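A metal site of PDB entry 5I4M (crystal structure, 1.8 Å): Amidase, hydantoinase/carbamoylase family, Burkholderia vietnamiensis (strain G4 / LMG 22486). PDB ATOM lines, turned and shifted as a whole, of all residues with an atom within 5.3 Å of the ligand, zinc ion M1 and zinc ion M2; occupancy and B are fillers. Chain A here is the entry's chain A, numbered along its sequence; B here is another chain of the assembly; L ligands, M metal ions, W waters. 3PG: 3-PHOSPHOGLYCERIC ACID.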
ATOM      1  N   SER A 103      -4.193   8.356 -21.466  1.00  0.00           N
ATOM      2  CA  SER A 103      -4.958   8.585 -20.250  1.00  0.00           C
ATOM      3  C   SER A 103      -5.378   7.220 -19.723  1.00  0.00           C
ATOM      4  O   SER A 103      -4.655   6.240 -19.881  1.00  0.00           O
ATOM      5  CB  SER A 103      -6.151   9.506 -20.566  1.00  0.00           C
ATOM      6  OG  SER A 103      -6.675  10.146 -19.391  1.00  0.00           O
ATOM      7  N   HIS A 104      -6.557   7.131 -19.109  1.00  0.00           N
ATOM      8  CA  HIS A 104      -7.008   5.884 -18.520  1.00  0.00           C
ATOM      9  C   HIS A 104      -8.349   5.473 -19.086  1.00  0.00           C
ATOM     10  O   HIS A 104      -9.202   6.314 -19.402  1.00  0.00           O
ATOM     11  CB  HIS A 104      -7.099   5.992 -16.992  1.00  0.00           C
ATOM     12  CG  HIS A 104      -7.974   7.109 -16.518  1.00  0.00           C
ATOM     13  ND1 HIS A 104      -9.263   6.900 -16.074  1.00  0.00           N
ATOM     14  CD2 HIS A 104      -7.745   8.434 -16.392  1.00  0.00           C
ATOM     15  CE1 HIS A 104      -9.794   8.054 -15.707  1.00  0.00           C
ATOM     16  NE2 HIS A 104      -8.890   8.999 -15.886  1.00  0.00           N
ATOM     17  N   GLN A 108     -14.636   5.286 -12.245  1.00  0.00           N
ATOM     18  CA  GLN A 108     -15.254   5.167 -10.947  1.00  0.00           C
ATOM     19  C   GLN A 108     -16.522   4.315 -11.056  1.00  0.00           C
ATOM     20  O   GLN A 108     -17.048   4.123 -12.154  1.00  0.00           O
ATOM     21  CB  GLN A 108     -15.610   6.553 -10.419  1.00  0.00           C
ATOM     22  CG  GLN A 108     -14.408   7.400 -10.181  1.00  0.00           C
ATOM     23  CD  GLN A 108     -13.756   7.033  -8.866  1.00  0.00           C
ATOM     24  OE1 GLN A 108     -14.415   6.472  -7.991  1.00  0.00           O
ATOM     25  NE2 GLN A 108     -12.463   7.324  -8.729  1.00  0.00           N
ATOM     26  N   ASP A 115     -14.327  11.038 -18.454  1.00  0.00           N
ATOM     27  CA  ASP A 115     -13.137  11.060 -17.597  1.00  0.00           C
ATOM     28  C   ASP A 115     -12.185   9.956 -18.033  1.00  0.00           C
ATOM     29  O   ASP A 115     -12.579   8.783 -18.123  1.00  0.00           O
ATOM     30  CB  ASP A 115     -13.576  10.898 -16.134  1.00  0.00           C
ATOM     31  CG  ASP A 115     -12.427  10.815 -15.149  1.00  0.00           C
ATOM     32  OD1 ASP A 115     -11.250  11.027 -15.509  1.00  0.00           O
ATOM     33  OD2 ASP A 115     -12.745  10.580 -13.945  1.00  0.00           O
ATOM     34  N   GLY A 116     -10.958  10.338 -18.378  1.00  0.00           N
ATOM     35  CA  GLY A 116      -9.975   9.379 -18.842  1.00  0.00           C
ATOM     36  C   GLY A 116     -10.138   8.882 -20.268  1.00  0.00           C
ATOM     37  O   GLY A 116      -9.214   8.974 -21.073  1.00  0.00           O
ATOM     38  N   GLU A 149      -5.872   4.077 -13.076  1.00  0.00           N
ATOM     39  CA  GLU A 149      -5.544   5.451 -12.749  1.00  0.00           C
ATOM     40  C   GLU A 149      -6.425   5.984 -11.616  1.00  0.00           C
ATOM     41  O   GLU A 149      -5.964   6.825 -10.843  1.00  0.00           O
ATOM     42  CB  GLU A 149      -5.645   6.352 -13.992  1.00  0.00           C
ATOM     43  CG  GLU A 149      -5.222   7.807 -13.780  1.00  0.00           C
ATOM     44  CD  GLU A 149      -6.330   8.681 -13.198  1.00  0.00           C
ATOM     45  OE1 GLU A 149      -7.486   8.219 -13.140  1.00  0.00           O
ATOM     46  OE2 GLU A 149      -6.027   9.817 -12.796  1.00  0.00           O
ATOM     47  N   GLU A 150      -7.663   5.492 -11.486  1.00  0.00           N
ATOM     48  CA  GLU A 150      -8.608   6.145 -10.580  1.00  0.00           C
ATOM     49  C   GLU A 150      -8.239   5.920  -9.115  1.00  0.00           C
ATOM     50  O   GLU A 150      -8.594   6.744  -8.258  1.00  0.00           O
ATOM     51  CB  GLU A 150     -10.032   5.664 -10.820  1.00  0.00           C
ATOM     52  CG  GLU A 150     -10.691   6.183 -12.104  1.00  0.00           C
ATOM     53  CD  GLU A 150     -11.170   7.625 -11.996  1.00  0.00           C
ATOM     54  OE1 GLU A 150     -10.878   8.287 -10.985  1.00  0.00           O
ATOM     55  OE2 GLU A 150     -11.853   8.109 -12.929  1.00  0.00           O
ATOM     56  N   ALA A 157      -4.322   6.289  -6.391  1.00  0.00           N
ATOM     57  CA  ALA A 157      -4.435   6.630  -7.802  1.00  0.00           C
ATOM     58  C   ALA A 157      -3.070   6.649  -8.484  1.00  0.00           C
ATOM     59  O   ALA A 157      -2.029   6.751  -7.845  1.00  0.00           O
ATOM     60  CB  ALA A 157      -5.094   7.994  -7.961  1.00  0.00           C
ATOM     61  N   MET A 158      -3.109   6.547  -9.815  1.00  0.00           N
ATOM     62  CA  MET A 158      -1.970   6.863 -10.670  1.00  0.00           C
ATOM     63  C   MET A 158      -0.761   5.962 -10.398  1.00  0.00           C
ATOM     64  O   MET A 158       0.384   6.360 -10.642  1.00  0.00           O
ATOM     65  CB  MET A 158      -1.583   8.334 -10.516  1.00  0.00           C
ATOM     66  CG  MET A 158      -2.697   9.306 -10.924  1.00  0.00           C
ATOM     67  SD  MET A 158      -2.730  10.804  -9.903  1.00  0.00           S
ATOM     68  CE  MET A 158      -1.055  11.398 -10.101  1.00  0.00           C
ATOM     69  N   HIS A 211      -7.889  15.979 -21.303  1.00  0.00           N
ATOM     70  CA  HIS A 211      -8.816  15.541 -20.250  1.00  0.00           C
ATOM     71  C   HIS A 211      -9.916  16.577 -20.078  1.00  0.00           C
ATOM     72  O   HIS A 211      -9.714  17.766 -20.362  1.00  0.00           O
ATOM     73  CB  HIS A 211      -8.067  15.369 -18.925  1.00  0.00           C
ATOM     74  CG  HIS A 211      -8.697  14.382 -17.994  1.00  0.00           C
ATOM     75  ND1 HIS A 211      -9.845  14.653 -17.278  1.00  0.00           N
ATOM     76  CD2 HIS A 211      -8.318  13.134 -17.628  1.00  0.00           C
ATOM     77  CE1 HIS A 211     -10.145  13.612 -16.520  1.00  0.00           C
ATOM     78  NE2 HIS A 211      -9.232  12.678 -16.715  1.00  0.00           N
ATOM     79  N   GLN A 214     -13.250  18.569 -15.185  1.00  0.00           N
ATOM     80  CA  GLN A 214     -13.822  17.993 -13.975  1.00  0.00           C
ATOM     81  C   GLN A 214     -14.184  19.058 -12.936  1.00  0.00           C
ATOM     82  O   GLN A 214     -14.412  18.740 -11.770  1.00  0.00           O
ATOM     83  CB  GLN A 214     -12.902  16.934 -13.350  1.00  0.00           C
ATOM     84  CG  GLN A 214     -12.568  15.830 -14.350  1.00  0.00           C
ATOM     85  CD  GLN A 214     -11.641  14.801 -13.758  1.00  0.00           C
ATOM     86  OE1 GLN A 214     -10.459  15.093 -13.551  1.00  0.00           O
ATOM     87  NE2 GLN A 214     -12.155  13.605 -13.492  1.00  0.00           N
ATOM     88  N   GLN A 234      -1.755  16.315  -3.632  1.00  0.00           N
ATOM     89  CA  GLN A 234      -2.723  15.504  -2.905  1.00  0.00           C
ATOM     90  C   GLN A 234      -2.042  14.715  -1.797  1.00  0.00           C
ATOM     91  O   GLN A 234      -0.873  14.341  -1.905  1.00  0.00           O
ATOM     92  CB  GLN A 234      -3.440  14.515  -3.822  1.00  0.00           C
ATOM     93  CG  GLN A 234      -4.060  15.114  -5.071  1.00  0.00           C
ATOM     94  CD  GLN A 234      -5.108  14.197  -5.680  1.00  0.00           C
ATOM     95  OE1 GLN A 234      -6.005  13.735  -4.980  1.00  0.00           O
ATOM     96  NE2 GLN A 234      -4.987  13.915  -6.969  1.00  0.00           N
ATOM     97  N   TRP A 236      -3.551  11.344   0.493  1.00  0.00           N
ATOM     98  CA  TRP A 236      -4.634  10.422   0.815  1.00  0.00           C
ATOM     99  C   TRP A 236      -4.263   9.596   2.043  1.00  0.00           C
ATOM    100  O   TRP A 236      -3.104   9.238   2.242  1.00  0.00           O
ATOM    101  CB  TRP A 236      -4.933   9.452  -0.333  1.00  0.00           C
ATOM    102  CG  TRP A 236      -5.460  10.065  -1.598  1.00  0.00           C
ATOM    103  CD1 TRP A 236      -5.506  11.385  -1.933  1.00  0.00           C
ATOM    104  CD2 TRP A 236      -6.022   9.342  -2.697  1.00  0.00           C
ATOM    105  NE1 TRP A 236      -6.072  11.533  -3.190  1.00  0.00           N
ATOM    106  CE2 TRP A 236      -6.382  10.290  -3.676  1.00  0.00           C
ATOM    107  CE3 TRP A 236      -6.245   7.978  -2.953  1.00  0.00           C
ATOM    108  CZ2 TRP A 236      -6.969   9.924  -4.898  1.00  0.00           C
ATOM    109  CZ3 TRP A 236      -6.828   7.611  -4.145  1.00  0.00           C
ATOM    110  CH2 TRP A 236      -7.190   8.578  -5.113  1.00  0.00           C
ATOM    111  N   ASP A 307      -9.151  12.401   1.884  1.00  0.00           N
ATOM    112  CA  ASP A 307      -8.654  12.925   0.614  1.00  0.00           C
ATOM    113  C   ASP A 307      -8.424  14.416   0.827  1.00  0.00           C
ATOM    114  O   ASP A 307      -9.381  15.153   1.093  1.00  0.00           O
ATOM    115  CB  ASP A 307      -9.673  12.663  -0.495  1.00  0.00           C
ATOM    116  CG  ASP A 307      -9.235  13.173  -1.874  1.00  0.00           C
ATOM    117  OD1 ASP A 307      -8.885  14.351  -2.024  1.00  0.00           O
ATOM    118  OD2 ASP A 307      -9.284  12.350  -2.813  1.00  0.00           O
ATOM    119  N   ARG A 309      -6.382  17.932  -0.791  1.00  0.00           N
ATOM    120  CA  ARG A 309      -5.686  18.502  -1.952  1.00  0.00           C
ATOM    121  C   ARG A 309      -5.512  20.001  -1.749  1.00  0.00           C
ATOM    122  O   ARG A 309      -6.369  20.667  -1.158  1.00  0.00           O
ATOM    123  CB  ARG A 309      -6.476  18.266  -3.249  1.00  0.00           C
ATOM    124  CG  ARG A 309      -7.106  16.884  -3.309  1.00  0.00           C
ATOM    125  CD  ARG A 309      -7.814  16.644  -4.629  1.00  0.00           C
ATOM    126  NE  ARG A 309      -8.437  15.324  -4.590  1.00  0.00           N
ATOM    127  CZ  ARG A 309      -8.662  14.579  -5.656  1.00  0.00           C
ATOM    128  NH1 ARG A 309      -8.335  15.024  -6.866  1.00  0.00           N
ATOM    129  NH2 ARG A 309      -9.181  13.363  -5.518  1.00  0.00           N
ATOM    130  N   TYR A 346       1.719  13.444  -3.384  1.00  0.00           N
ATOM    131  CA  TYR A 346       2.631  14.089  -4.323  1.00  0.00           C
ATOM    132  C   TYR A 346       2.457  15.596  -4.239  1.00  0.00           C
ATOM    133  O   TYR A 346       1.346  16.093  -3.998  1.00  0.00           O
ATOM    134  CB  TYR A 346       2.438  13.596  -5.769  1.00  0.00           C
ATOM    135  CG  TYR A 346       1.104  13.899  -6.413  1.00  0.00           C
ATOM    136  CD1 TYR A 346       0.915  15.077  -7.137  1.00  0.00           C
ATOM    137  CD2 TYR A 346       0.051  12.985  -6.356  1.00  0.00           C
ATOM    138  CE1 TYR A 346      -0.300  15.358  -7.760  1.00  0.00           C
ATOM    139  CE2 TYR A 346      -1.162  13.255  -6.970  1.00  0.00           C
ATOM    140  CZ  TYR A 346      -1.336  14.433  -7.655  1.00  0.00           C
ATOM    141  OH  TYR A 346      -2.542  14.680  -8.264  1.00  0.00           O
ATOM    142  N   GLY A 376      -7.319  20.234 -10.837  1.00  0.00           N
ATOM    143  CA  GLY A 376      -7.725  19.923  -9.481  1.00  0.00           C
ATOM    144  C   GLY A 376      -7.671  18.440  -9.210  1.00  0.00           C
ATOM    145  O   GLY A 376      -7.600  18.001  -8.058  1.00  0.00           O
ATOM    146  N   ALA A 377      -7.721  17.637 -10.276  1.00  0.00           N
ATOM    147  CA  ALA A 377      -7.562  16.197 -10.164  1.00  0.00           C
ATOM    148  C   ALA A 377      -6.121  15.807 -10.454  1.00  0.00           C
ATOM    149  O   ALA A 377      -5.334  16.590 -10.985  1.00  0.00           O
ATOM    150  CB  ALA A 377      -8.506  15.468 -11.124  1.00  0.00           C
ATOM    151  N   GLY A 378      -5.792  14.580 -10.084  1.00  0.00           N
ATOM    152  CA  GLY A 378      -4.544  13.974 -10.510  1.00  0.00           C
ATOM    153  C   GLY A 378      -4.721  13.276 -11.846  1.00  0.00           C
ATOM    154  O   GLY A 378      -5.822  12.822 -12.187  1.00  0.00           O
ATOM    155  N   HIS A 379      -3.641  13.201 -12.606  1.00  0.00           N
ATOM    156  CA  HIS A 379      -3.626  12.534 -13.889  1.00  0.00           C
ATOM    157  C   HIS A 379      -2.306  11.821 -14.047  1.00  0.00           C
ATOM    158  O   HIS A 379      -1.312  12.177 -13.414  1.00  0.00           O
ATOM    159  CB  HIS A 379      -3.831  13.522 -15.033  1.00  0.00           C
ATOM    160  CG  HIS A 379      -5.004  14.410 -14.825  1.00  0.00           C
ATOM    161  ND1 HIS A 379      -6.295  13.994 -15.078  1.00  0.00           N
ATOM    162  CD2 HIS A 379      -5.100  15.676 -14.354  1.00  0.00           C
ATOM    163  CE1 HIS A 379      -7.127  14.968 -14.784  1.00  0.00           C
ATOM    164  NE2 HIS A 379      -6.437  15.997 -14.349  1.00  0.00           N
ATOM    165  N   SER A 402     -17.978  15.726 -12.419  1.00  0.00           N
ATOM    166  CA  SER A 402     -17.291  14.502 -12.794  1.00  0.00           C
ATOM    167  C   SER A 402     -17.421  13.547 -11.619  1.00  0.00           C
ATOM    168  O   SER A 402     -17.831  13.939 -10.522  1.00  0.00           O
ATOM    169  CB  SER A 402     -15.830  14.760 -13.163  1.00  0.00           C
ATOM    170  OG  SER A 402     -15.205  13.580 -13.613  1.00  0.00           O
ATOM    171  N   HIS A 403     -17.101  12.286 -11.862  1.00  0.00           N
ATOM    172  CA  HIS A 403     -17.310  11.202 -10.894  1.00  0.00           C
ATOM    173  C   HIS A 403     -18.783  11.061 -10.533  1.00  0.00           C
ATOM    174  O   HIS A 403     -19.129  10.617  -9.435  1.00  0.00           O
ATOM    175  CB  HIS A 403     -16.417  11.380  -9.666  1.00  0.00           C
ATOM    176  CG  HIS A 403     -14.975  11.043  -9.950  1.00  0.00           C
ATOM    177  ND1 HIS A 403     -14.024  10.891  -8.961  1.00  0.00           N
ATOM    178  CD2 HIS A 403     -14.348  10.817 -11.130  1.00  0.00           C
ATOM    179  CE1 HIS A 403     -12.873  10.580  -9.518  1.00  0.00           C
ATOM    180  NE2 HIS A 403     -13.037  10.524 -10.831  1.00  0.00           N
ATOM    181  N   HIS B 247     -16.750  14.819  -7.893  1.00  0.00           N
ATOM    182  CA  HIS B 247     -15.322  14.579  -7.724  1.00  0.00           C
ATOM    183  C   HIS B 247     -14.839  15.125  -6.374  1.00  0.00           C
ATOM    184  O   HIS B 247     -15.173  16.243  -5.978  1.00  0.00           O
ATOM    185  CB  HIS B 247     -14.532  15.248  -8.852  1.00  0.00           C
ATOM    186  CG  HIS B 247     -13.230  14.589  -9.116  1.00  0.00           C
ATOM    187  ND1 HIS B 247     -12.199  14.578  -8.204  1.00  0.00           N
ATOM    188  CD2 HIS B 247     -12.788  13.867 -10.180  1.00  0.00           C
ATOM    189  CE1 HIS B 247     -11.176  13.894  -8.694  1.00  0.00           C
ATOM    190  NE2 HIS B 247     -11.513  13.457  -9.896  1.00  0.00           N
ATOM    191  N   ASN B 296     -12.297   8.758  -3.700  1.00  0.00           N
ATOM    192  CA  ASN B 296     -12.232  10.045  -4.376  1.00  0.00           C
ATOM    193  C   ASN B 296     -13.562  10.433  -5.034  1.00  0.00           C
ATOM    194  O   ASN B 296     -13.580  11.144  -6.037  1.00  0.00           O
ATOM    195  CB  ASN B 296     -11.048  10.118  -5.371  1.00  0.00           C
ATOM    196  CG  ASN B 296     -10.952   8.925  -6.326  1.00  0.00           C
ATOM    197  OD1 ASN B 296     -11.570   7.881  -6.145  1.00  0.00           O
ATOM    198  ND2 ASN B 296     -10.106   9.085  -7.358  1.00  0.00           N
HETATM  199  C1  3PG L   1      -8.030  11.939  -8.530  1.00  0.00           C
HETATM  200  O1  3PG L   1      -8.943  11.657  -7.734  1.00  0.00           O
HETATM  201  O2  3PG L   1      -7.680  13.121  -8.761  1.00  0.00           O
HETATM  202  C2  3PG L   1      -7.324  10.808  -9.223  1.00  0.00           C
HETATM  203  O3  3PG L   1      -6.033  11.241  -9.698  1.00  0.00           O
HETATM  204  C3  3PG L   1      -8.168  10.378 -10.401  1.00  0.00           C
HETATM  205  O1P 3PG L   1      -8.235  11.447 -11.349  1.00  0.00           O
HETATM  206  P   3PG L   1      -9.385  11.412 -12.517  1.00  0.00           P
HETATM  207  O2P 3PG L   1      -9.384  10.009 -13.073  1.00  0.00           O
HETATM  208  O3P 3PG L   1     -10.668  11.738 -11.772  1.00  0.00           O
HETATM  209  O4P 3PG L   1      -8.897  12.472 -13.525  1.00  0.00           O
HETATM  210 ZN    ZN M   1      -9.150  11.041 -15.181  1.00  0.00          ZN
HETATM  211 ZN    ZN M   2     -11.603  10.073 -12.359  1.00  0.00          ZN
HETATM  212  O   HOH W   1      -6.970  11.253 -15.187  1.00  0.00           O
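Gln 214 touches zinc ion M2 (NE2 to ZN, 3.8 Å). Within 4 Å of zinc ion M2: Asp 115, Glu 150, Gln 214 and His 403.
OD1 of Asp 115 binds zinc ion M1 (2.1 Å). Zinc ion M1 is bound by NE2 of His 104 (2.2 Å). Water W1 is bound to zinc ion M1. Zinc ion M1 is bound by O4P of the ligand, at 2.2 Å. A ring nitrogen (NE2) of His 211 binds zinc ion M1, at 2.2 Å. An oxygen (O2P) of the ligand is bound to zinc ion M1 (2.4 Å). Zinc ion M1 has six donor atoms within binding distance.
The side-chain carboxylate (OE2) of Glu 149 sits close to an oxygen (O3) of the ligand, 3.4 Å away. A ring nitrogen (NE2) of His 247 of chain B sits close to an oxygen (O3P) of the ligand (2.7 Å). The backbone NH of Gly 378 lies within hydrogen-bond range of an oxygen (O2) of the ligand, 2.7 Å away. The backbone carbonyl oxygen (O) of Gly 378 sits at hydrogen-bond distance from an oxygen (O3) of the ligand (3.0 Å). An oxygen (O2) of the ligand is in salt-bridge range of the guanidinium group (NH1) of Arg 309, 2.8 Å away. ND2 of Asn 296 of chain B sits at hydrogen-bond distance from O1 of the ligand (2.8 Å). An oxygen (O3P) of the ligand sits close to the side-chain amide nitrogen of Gln 214, 2.9 Å away. A ring nitrogen (ND1) of His 379 sits close to an oxygen (O4P) of the ligand (3.4 Å). NE2 of Gln 234 sits at hydrogen-bond distance from O2 of the ligand. An oxygen (O3) of the ligand lies within hydrogen-bond range of the side-chain sulfur (SD) of Met 158, at 3.3 Å.
Zinc ion M2 is bound by O3P of the ligand (2.0 Å), OD2 of Asp 115 (2.0 Å), OE2 of Glu 150 (2.1 Å), NE2 of His 403 (2.1 Å), O2P of the ligand (2.3 Å) and OE1 of Glu 150 (2.4 Å). Zinc ion M2 has six donor atoms within binding distance.
Ala 157 touches the ligand. CZ2 of Trp 236 touches O1 of the ligand, 3.9 Å away. CA of Ala 377 touches O2 of the ligand (3.4 Å). Hydrophobic or aromatic side chains that line the ligand: His 104, Ala 157, Met 158, His 211, Trp 236, Ala 377, His 379, His 403 and His 247 of chain B. 17 residues have an atom within 4 Å of the ligand: His 104, Asp 115, Glu 149, Glu 150, Ala 157, Met 158, His 211, Gln 214, Gln 234, Trp 236, Arg 309, Ala 377, Gly 378, His 379, His 403, His 247 of chain B and Asn 296 of chain B.
OE1 of Glu 150 sits close to NE2 of Gln 108 (2.9 Å). The backbone carbonyl oxygen (O) of Asn 296 of chain B lies within hydrogen-bond range of a ring nitrogen (ND1) of His 403 (3.0 Å). A ring nitrogen (NE2) of His 104 sits close to the side-chain carboxylate (OE1) of Glu 149. The backbone NH (N) of Gly 116 lies close to a ring nitrogen (NE2) of His 211 (3.3 Å). OG of Ser 402 lies within hydrogen-bond range of NE2 of Gln 214 (3.1 Å). The side-chain amide nitrogen of Gln 234 sits at hydrogen-bond distance from the side-chain hydroxyl of Tyr 346 (2.9 Å). The backbone carbonyl oxygen (O) of Gly 116 lies close to the side-chain hydroxyl (OG) of Ser 103 (3.3 Å). NE1 of Trp 236 sits at hydrogen-bond distance from OD2 of Asp 307 (3.3 Å).
Merely in contact with zinc ion M1: Gly 116 and Glu 149. Of the 24 residues printed, 5 come within 4 Å of zinc ion M1.
Water W1 bridges a ring nitrogen (ND1) of His 379 and the side-chain carboxylate of Glu 149.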
